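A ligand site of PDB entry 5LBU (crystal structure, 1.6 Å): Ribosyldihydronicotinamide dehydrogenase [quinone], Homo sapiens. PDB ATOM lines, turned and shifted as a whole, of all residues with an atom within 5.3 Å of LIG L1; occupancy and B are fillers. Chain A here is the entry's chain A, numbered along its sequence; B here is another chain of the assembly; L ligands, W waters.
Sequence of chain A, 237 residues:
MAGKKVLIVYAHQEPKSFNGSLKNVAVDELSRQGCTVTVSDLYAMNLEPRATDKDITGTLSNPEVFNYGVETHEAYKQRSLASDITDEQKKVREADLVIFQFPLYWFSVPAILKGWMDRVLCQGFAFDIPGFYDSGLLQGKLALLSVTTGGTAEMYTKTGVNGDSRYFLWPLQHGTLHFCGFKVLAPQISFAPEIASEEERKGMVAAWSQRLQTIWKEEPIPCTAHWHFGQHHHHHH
O1 of LIG L1 lies close to OD1 of Asn 162.
N of Gly 151 lies within hydrogen-bond range of N2 of LIG L1.
O7 of LG2 L2 lies within hydrogen-bond range of N of Gly 151 (3.1 Å).
The backbone NH of Gly 150 is in hydrogen-bond range of a nitrogen (N6) of LG2 L2, 3.1 Å away.
The backbone NH of Trp 106 sits at hydrogen-bond distance from a nitrogen (N8) of LG2 L2 (2.9 Å).
The side-chain hydroxyl (OH) of Tyr 156 is in hydrogen-bond range of an oxygen (O7) of LG2 L2 (2.7 Å).
OE1 of Glu 194 is in hydrogen-bond range of O10 of LG2 L2 (2.6 Å).
Residues that only touch LIG L1: Met 155 (3.2 Å), Phe 127 of chain B (3.3 Å), Gly 150 (3.5 Å), Trp 106 (3.6 Å), Phe 179 of chain B (3.6 Å), Phe 132 of chain B (3.6 Å) and Ile 129 of chain B (3.7 Å).
Of the 12 residues printed, 9 come within 4 Å of LIG L1.
Water W1 bridges a nitrogen (N3) of LIG L1 (2.7 Å) and the side-chain amide nitrogen of Asn 162 (3.1 Å).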
ATOM      1  N   TRP A 106      25.746  34.910  15.317  1.00  0.00           N
ATOM      2  CA  TRP A 106      25.599  36.239  14.715  1.00  0.00           C
ATOM      3  C   TRP A 106      26.646  37.235  15.248  1.00  0.00           C
ATOM      4  O   TRP A 106      26.312  38.318  15.759  1.00  0.00           O
ATOM      5  CB  TRP A 106      24.160  36.744  14.899  1.00  0.00           C
ATOM      6  CG  TRP A 106      23.183  35.963  14.092  1.00  0.00           C
ATOM      7  CD1 TRP A 106      22.111  35.247  14.557  1.00  0.00           C
ATOM      8  CD2 TRP A 106      23.212  35.776  12.679  1.00  0.00           C
ATOM      9  NE1 TRP A 106      21.465  34.638  13.509  1.00  0.00           N
ATOM     10  CE2 TRP A 106      22.122  34.948  12.342  1.00  0.00           C
ATOM     11  CE3 TRP A 106      24.047  36.238  11.654  1.00  0.00           C
ATOM     12  CZ2 TRP A 106      21.848  34.579  11.029  1.00  0.00           C
ATOM     13  CZ3 TRP A 106      23.780  35.864  10.348  1.00  0.00           C
ATOM     14  CH2 TRP A 106      22.694  35.034  10.054  1.00  0.00           C
ATOM     15  N   GLY A 150      31.752  28.908  13.191  1.00  0.00           N
ATOM     16  CA  GLY A 150      31.524  28.192  11.941  1.00  0.00           C
ATOM     17  C   GLY A 150      32.641  28.470  10.951  1.00  0.00           C
ATOM     18  O   GLY A 150      33.098  27.566  10.265  1.00  0.00           O
ATOM     19  N   GLY A 151      33.081  29.726  10.893  1.00  0.00           N
ATOM     20  CA  GLY A 151      34.134  30.156   9.958  1.00  0.00           C
ATOM     21  C   GLY A 151      35.552  29.762  10.351  1.00  0.00           C
ATOM     22  O   GLY A 151      35.886  29.648  11.536  1.00  0.00           O
ATOM     23  N   MET A 155      39.204  32.972   7.148  1.00  0.00           N
ATOM     24  CA  MET A 155      38.027  33.821   6.868  1.00  0.00           C
ATOM     25  C   MET A 155      37.872  35.014   7.805  1.00  0.00           C
ATOM     26  O   MET A 155      37.208  35.997   7.459  1.00  0.00           O
ATOM     27  CB  MET A 155      36.744  32.999   6.944  1.00  0.00           C
ATOM     28  CG  MET A 155      36.691  31.848   5.965  1.00  0.00           C
ATOM     29  SD  MET A 155      35.264  30.835   6.364  1.00  0.00           S
ATOM     30  CE  MET A 155      34.030  31.649   5.366  1.00  0.00           C
ATOM     31  N   TYR A 156      38.461  34.914   8.991  1.00  0.00           N
ATOM     32  CA  TYR A 156      38.387  35.958  10.008  1.00  0.00           C
ATOM     33  C   TYR A 156      39.668  36.813  10.010  1.00  0.00           C
ATOM     34  O   TYR A 156      40.279  37.045  11.049  1.00  0.00           O
ATOM     35  CB  TYR A 156      38.036  35.335  11.384  1.00  0.00           C
ATOM     36  CG  TYR A 156      36.548  35.012  11.539  1.00  0.00           C
ATOM     37  CD1 TYR A 156      35.620  36.044  11.600  1.00  0.00           C
ATOM     38  CD2 TYR A 156      36.067  33.688  11.622  1.00  0.00           C
ATOM     39  CE1 TYR A 156      34.265  35.800  11.740  1.00  0.00           C
ATOM     40  CE2 TYR A 156      34.694  33.441  11.745  1.00  0.00           C
ATOM     41  CZ  TYR A 156      33.801  34.495  11.802  1.00  0.00           C
ATOM     42  OH  TYR A 156      32.424  34.329  11.926  1.00  0.00           O
ATOM     43  N   ASN A 162      34.467  38.346   6.357  1.00  0.00           N
ATOM     44  CA  ASN A 162      33.985  38.465   7.739  1.00  0.00           C
ATOM     45  C   ASN A 162      34.684  39.539   8.561  1.00  0.00           C
ATOM     46  O   ASN A 162      34.155  39.964   9.582  1.00  0.00           O
ATOM     47  CB  ASN A 162      34.088  37.133   8.487  1.00  0.00           C
ATOM     48  CG  ASN A 162      33.085  36.081   8.013  1.00  0.00           C
ATOM     49  OD1 ASN A 162      33.426  34.901   7.936  1.00  0.00           O
ATOM     50  ND2 ASN A 162      31.845  36.487   7.753  1.00  0.00           N
ATOM     51  N   GLU A 194      33.363  22.076  13.250  1.00  0.00           N
ATOM     52  CA  GLU A 194      32.504  21.242  12.407  1.00  0.00           C
ATOM     53  C   GLU A 194      33.185  20.890  11.094  1.00  0.00           C
ATOM     54  O   GLU A 194      32.984  19.805  10.577  1.00  0.00           O
ATOM     55  CB  GLU A 194      31.174  21.921  12.126  1.00  0.00           C
ATOM     56  CG  GLU A 194      30.290  22.140  13.353  1.00  0.00           C
ATOM     57  CD  GLU A 194      29.193  23.157  13.101  1.00  0.00           C
ATOM     58  OE1 GLU A 194      29.512  24.361  13.000  1.00  0.00           O
ATOM     59  OE2 GLU A 194      28.024  22.753  12.998  1.00  0.00           O
ATOM     60  N   GLN B 123      19.334  29.072   8.563  1.00  0.00           N
ATOM     61  CA  GLN B 123      19.888  28.671   7.281  1.00  0.00           C
ATOM     62  C   GLN B 123      18.768  28.102   6.428  1.00  0.00           C
ATOM     63  O   GLN B 123      17.866  27.415   6.932  1.00  0.00           O
ATOM     64  CB  GLN B 123      21.013  27.652   7.452  1.00  0.00           C
ATOM     65  CG  GLN B 123      21.782  27.364   6.159  1.00  0.00           C
ATOM     66  CD  GLN B 123      23.050  26.570   6.402  1.00  0.00           C
ATOM     67  OE1 GLN B 123      23.440  26.326   7.524  1.00  0.00           O
ATOM     68  NE2 GLN B 123      23.706  26.181   5.320  1.00  0.00           N
ATOM     69  N   PHE B 127      19.933  32.807   4.819  1.00  0.00           N
ATOM     70  CA  PHE B 127      21.187  32.598   4.099  1.00  0.00           C
ATOM     71  C   PHE B 127      21.367  31.124   3.799  1.00  0.00           C
ATOM     72  O   PHE B 127      20.720  30.275   4.402  1.00  0.00           O
ATOM     73  CB  PHE B 127      22.346  33.056   4.974  1.00  0.00           C
ATOM     74  CG  PHE B 127      22.570  32.178   6.162  1.00  0.00           C
ATOM     75  CD1 PHE B 127      21.859  32.392   7.349  1.00  0.00           C
ATOM     76  CD2 PHE B 127      23.455  31.110   6.087  1.00  0.00           C
ATOM     77  CE1 PHE B 127      22.058  31.563   8.437  1.00  0.00           C
ATOM     78  CE2 PHE B 127      23.660  30.288   7.172  1.00  0.00           C
ATOM     79  CZ  PHE B 127      22.961  30.521   8.361  1.00  0.00           C
ATOM     80  N   ILE B 129      24.990  28.454   2.475  1.00  0.00           N
ATOM     81  CA  ILE B 129      26.440  28.398   2.299  1.00  0.00           C
ATOM     82  C   ILE B 129      26.684  27.492   1.091  1.00  0.00           C
ATOM     83  O   ILE B 129      26.563  26.285   1.226  1.00  0.00           O
ATOM     84  CB  ILE B 129      27.138  27.880   3.574  1.00  0.00           C
ATOM     85  CG1 ILE B 129      26.824  28.805   4.756  1.00  0.00           C
ATOM     86  CG2 ILE B 129      28.658  27.796   3.366  1.00  0.00           C
ATOM     87  CD1 ILE B 129      27.246  28.281   6.108  1.00  0.00           C
ATOM     88  N   PHE B 132      25.498  34.014   1.030  1.00  0.00           N
ATOM     89  CA  PHE B 132      25.631  34.994   2.105  1.00  0.00           C
ATOM     90  C   PHE B 132      26.214  36.331   1.639  1.00  0.00           C
ATOM     91  O   PHE B 132      26.651  36.455   0.512  1.00  0.00           O
ATOM     92  CB  PHE B 132      26.365  34.416   3.294  1.00  0.00           C
ATOM     93  CG  PHE B 132      27.670  33.820   2.935  1.00  0.00           C
ATOM     94  CD1 PHE B 132      28.779  34.608   2.836  1.00  0.00           C
ATOM     95  CD2 PHE B 132      27.770  32.478   2.674  1.00  0.00           C
ATOM     96  CE1 PHE B 132      29.998  34.067   2.495  1.00  0.00           C
ATOM     97  CE2 PHE B 132      28.982  31.930   2.336  1.00  0.00           C
ATOM     98  CZ  PHE B 132      30.089  32.724   2.245  1.00  0.00           C
ATOM     99  N   PHE B 179      25.010  39.865   6.147  1.00  0.00           N
ATOM    100  CA  PHE B 179      25.219  38.429   5.946  1.00  0.00           C
ATOM    101  C   PHE B 179      24.007  37.728   5.322  1.00  0.00           C
ATOM    102  O   PHE B 179      24.165  36.843   4.474  1.00  0.00           O
ATOM    103  CB  PHE B 179      25.611  37.742   7.270  1.00  0.00           C
ATOM    104  CG  PHE B 179      26.076  36.326   7.092  1.00  0.00           C
ATOM    105  CD1 PHE B 179      27.417  36.055   6.847  1.00  0.00           C
ATOM    106  CD2 PHE B 179      25.193  35.268   7.167  1.00  0.00           C
ATOM    107  CE1 PHE B 179      27.861  34.765   6.656  1.00  0.00           C
ATOM    108  CE2 PHE B 179      25.643  33.957   7.020  1.00  0.00           C
ATOM    109  CZ  PHE B 179      26.979  33.714   6.753  1.00  0.00           C
HETATM  110  N1  LIG L   1      28.840  27.333   9.515  1.00  0.00           N
HETATM  111  C1  LIG L   1      28.287  28.702   9.685  1.00  0.00           C
HETATM  112  C2  LIG L   1      29.124  29.860   9.304  1.00  0.00           C
HETATM  113  N2  LIG L   1      30.343  30.061   8.793  1.00  0.00           N
HETATM  114  C3  LIG L   1      30.514  31.403   8.676  1.00  0.00           C
HETATM  115  C4  LIG L   1      31.770  32.043   8.138  1.00  0.00           C
HETATM  116  O1  LIG L   1      31.513  32.879   6.984  1.00  0.00           O
HETATM  117  C5  LIG L   1      30.859  32.388   5.789  1.00  0.00           C
HETATM  118  C6  LIG L   1      30.555  30.911   5.660  1.00  0.00           C
HETATM  119  N3  LIG L   1      29.428  32.075   9.094  1.00  0.00           N
HETATM  120  C7  LIG L   1      28.532  31.185   9.482  1.00  0.00           C
HETATM  121  C8  LIG L   1      27.258  31.333   9.991  1.00  0.00           C
HETATM  122  C9  LIG L   1      26.697  32.591  10.166  1.00  0.00           C
HETATM  123  C10 LIG L   1      25.407  32.696  10.676  1.00  0.00           C
HETATM  124  C11 LIG L   1      24.679  31.561  11.025  1.00  0.00           C
HETATM  125  C12 LIG L   1      25.232  30.296  10.853  1.00  0.00           C
HETATM  126  C13 LIG L   1      26.521  30.173  10.330  1.00  0.00           C
HETATM  127  N4  LIG L   1      27.039  28.922  10.174  1.00  0.00           N
HETATM  128  P1  LG2 L   2      29.833  20.615  17.241  1.00  0.00           P
HETATM  129  O1  LG2 L   2      29.030  20.435  15.999  1.00  0.00           O
HETATM  130  O2  LG2 L   2      29.314  20.130  18.541  1.00  0.00           O
HETATM  131  O3  LG2 L   2      31.263  19.944  17.038  1.00  0.00           O
HETATM  132  C1  LG2 L   2      31.802  19.601  15.785  1.00  0.00           C
HETATM  133  C2  LG2 L   2      32.399  18.207  15.914  1.00  0.00           C
HETATM  134  O4  LG2 L   2      33.294  18.139  17.013  1.00  0.00           O
HETATM  135  C3  LG2 L   2      31.316  17.182  16.182  1.00  0.00           C
HETATM  136  O5  LG2 L   2      31.491  16.170  15.215  1.00  0.00           O
HETATM  137  C4  LG2 L   2      31.639  16.659  17.576  1.00  0.00           C
HETATM  138  O6  LG2 L   2      31.313  15.289  17.738  1.00  0.00           O
HETATM  139  C5  LG2 L   2      33.130  16.871  17.614  1.00  0.00           C
HETATM  140  N1  LG2 L   2      33.729  16.793  18.958  1.00  0.00           N
HETATM  141  C6  LG2 L   2      33.143  17.021  20.139  1.00  0.00           C
HETATM  142  N2  LG2 L   2      34.000  16.839  21.155  1.00  0.00           N
HETATM  143  C7  LG2 L   2      35.170  16.473  20.620  1.00  0.00           C
HETATM  144  C8  LG2 L   2      36.510  16.117  21.128  1.00  0.00           C
HETATM  145  N3  LG2 L   2      36.780  16.125  22.444  1.00  0.00           N
HETATM  146  N4  LG2 L   2      37.443  15.789  20.228  1.00  0.00           N
HETATM  147  C9  LG2 L   2      37.200  15.785  18.918  1.00  0.00           C
HETATM  148  N5  LG2 L   2      36.020  16.095  18.386  1.00  0.00           N
HETATM  149  C10 LG2 L   2      34.981  16.433  19.174  1.00  0.00           C
HETATM  150  N6  LG2 L   2      29.450  30.944  12.939  1.00  0.00           N
HETATM  151  C11 LG2 L   2      30.186  32.034  12.614  1.00  0.00           C
HETATM  152  O7  LG2 L   2      31.355  31.866  12.268  1.00  0.00           O
HETATM  153  N7  LG2 L   2      29.709  33.279  12.671  1.00  0.00           N
HETATM  154  C12 LG2 L   2      28.457  33.543  13.031  1.00  0.00           C
HETATM  155  O8  LG2 L   2      28.016  34.698  13.079  1.00  0.00           O
HETATM  156  C13 LG2 L   2      27.592  32.410  13.396  1.00  0.00           C
HETATM  157  N8  LG2 L   2      26.327  32.586  13.767  1.00  0.00           N
HETATM  158  C14 LG2 L   2      25.561  31.534  14.104  1.00  0.00           C
HETATM  159  C15 LG2 L   2      24.251  31.735  14.494  1.00  0.00           C
HETATM  160  C16 LG2 L   2      23.438  30.677  14.844  1.00  0.00           C
HETATM  161  C17 LG2 L   2      22.019  30.919  15.267  1.00  0.00           C
HETATM  162  C18 LG2 L   2      23.963  29.305  14.785  1.00  0.00           C
HETATM  163  C19 LG2 L   2      23.064  28.157  15.175  1.00  0.00           C
HETATM  164  C20 LG2 L   2      25.268  29.091  14.391  1.00  0.00           C
HETATM  165  C21 LG2 L   2      26.085  30.150  14.054  1.00  0.00           C
HETATM  166  N9  LG2 L   2      27.414  29.950  13.645  1.00  0.00           N
HETATM  167  C22 LG2 L   2      28.188  31.063  13.330  1.00  0.00           C
HETATM  168  C23 LG2 L   2      27.982  28.613  13.601  1.00  0.00           C
HETATM  169  C24 LG2 L   2      28.398  28.214  15.024  1.00  0.00           C
HETATM  170  O9  LG2 L   2      29.238  29.216  15.584  1.00  0.00           O
HETATM  171  C25 LG2 L   2      29.082  26.858  15.023  1.00  0.00           C
HETATM  172  O10 LG2 L   2      28.160  25.908  14.524  1.00  0.00           O
HETATM  173  C26 LG2 L   2      29.516  26.431  16.421  1.00  0.00           C
HETATM  174  O11 LG2 L   2      30.522  27.303  16.918  1.00  0.00           O
HETATM  175  C27 LG2 L   2      30.010  24.994  16.429  1.00  0.00           C
HETATM  176  O12 LG2 L   2      30.367  24.563  17.724  1.00  0.00           O
HETATM  177  P2  LG2 L   2      29.676  23.261  18.335  1.00  0.00           P
HETATM  178  O13 LG2 L   2      30.218  23.037  19.693  1.00  0.00           O
HETATM  179  O14 LG2 L   2      28.223  23.346  18.104  1.00  0.00           O
HETATM  180  O15 LG2 L   2      30.282  22.155  17.346  1.00  0.00           O
HETATM  181  O   HOH W   1      29.865  34.701   9.362  1.00  0.00           O
HETATM  182  O   HOH W   2      27.606  35.804  10.552  1.00  0.00           O
HETATM  183  O   HOH W   3      25.099  26.821  11.792  1.00  0.00           O
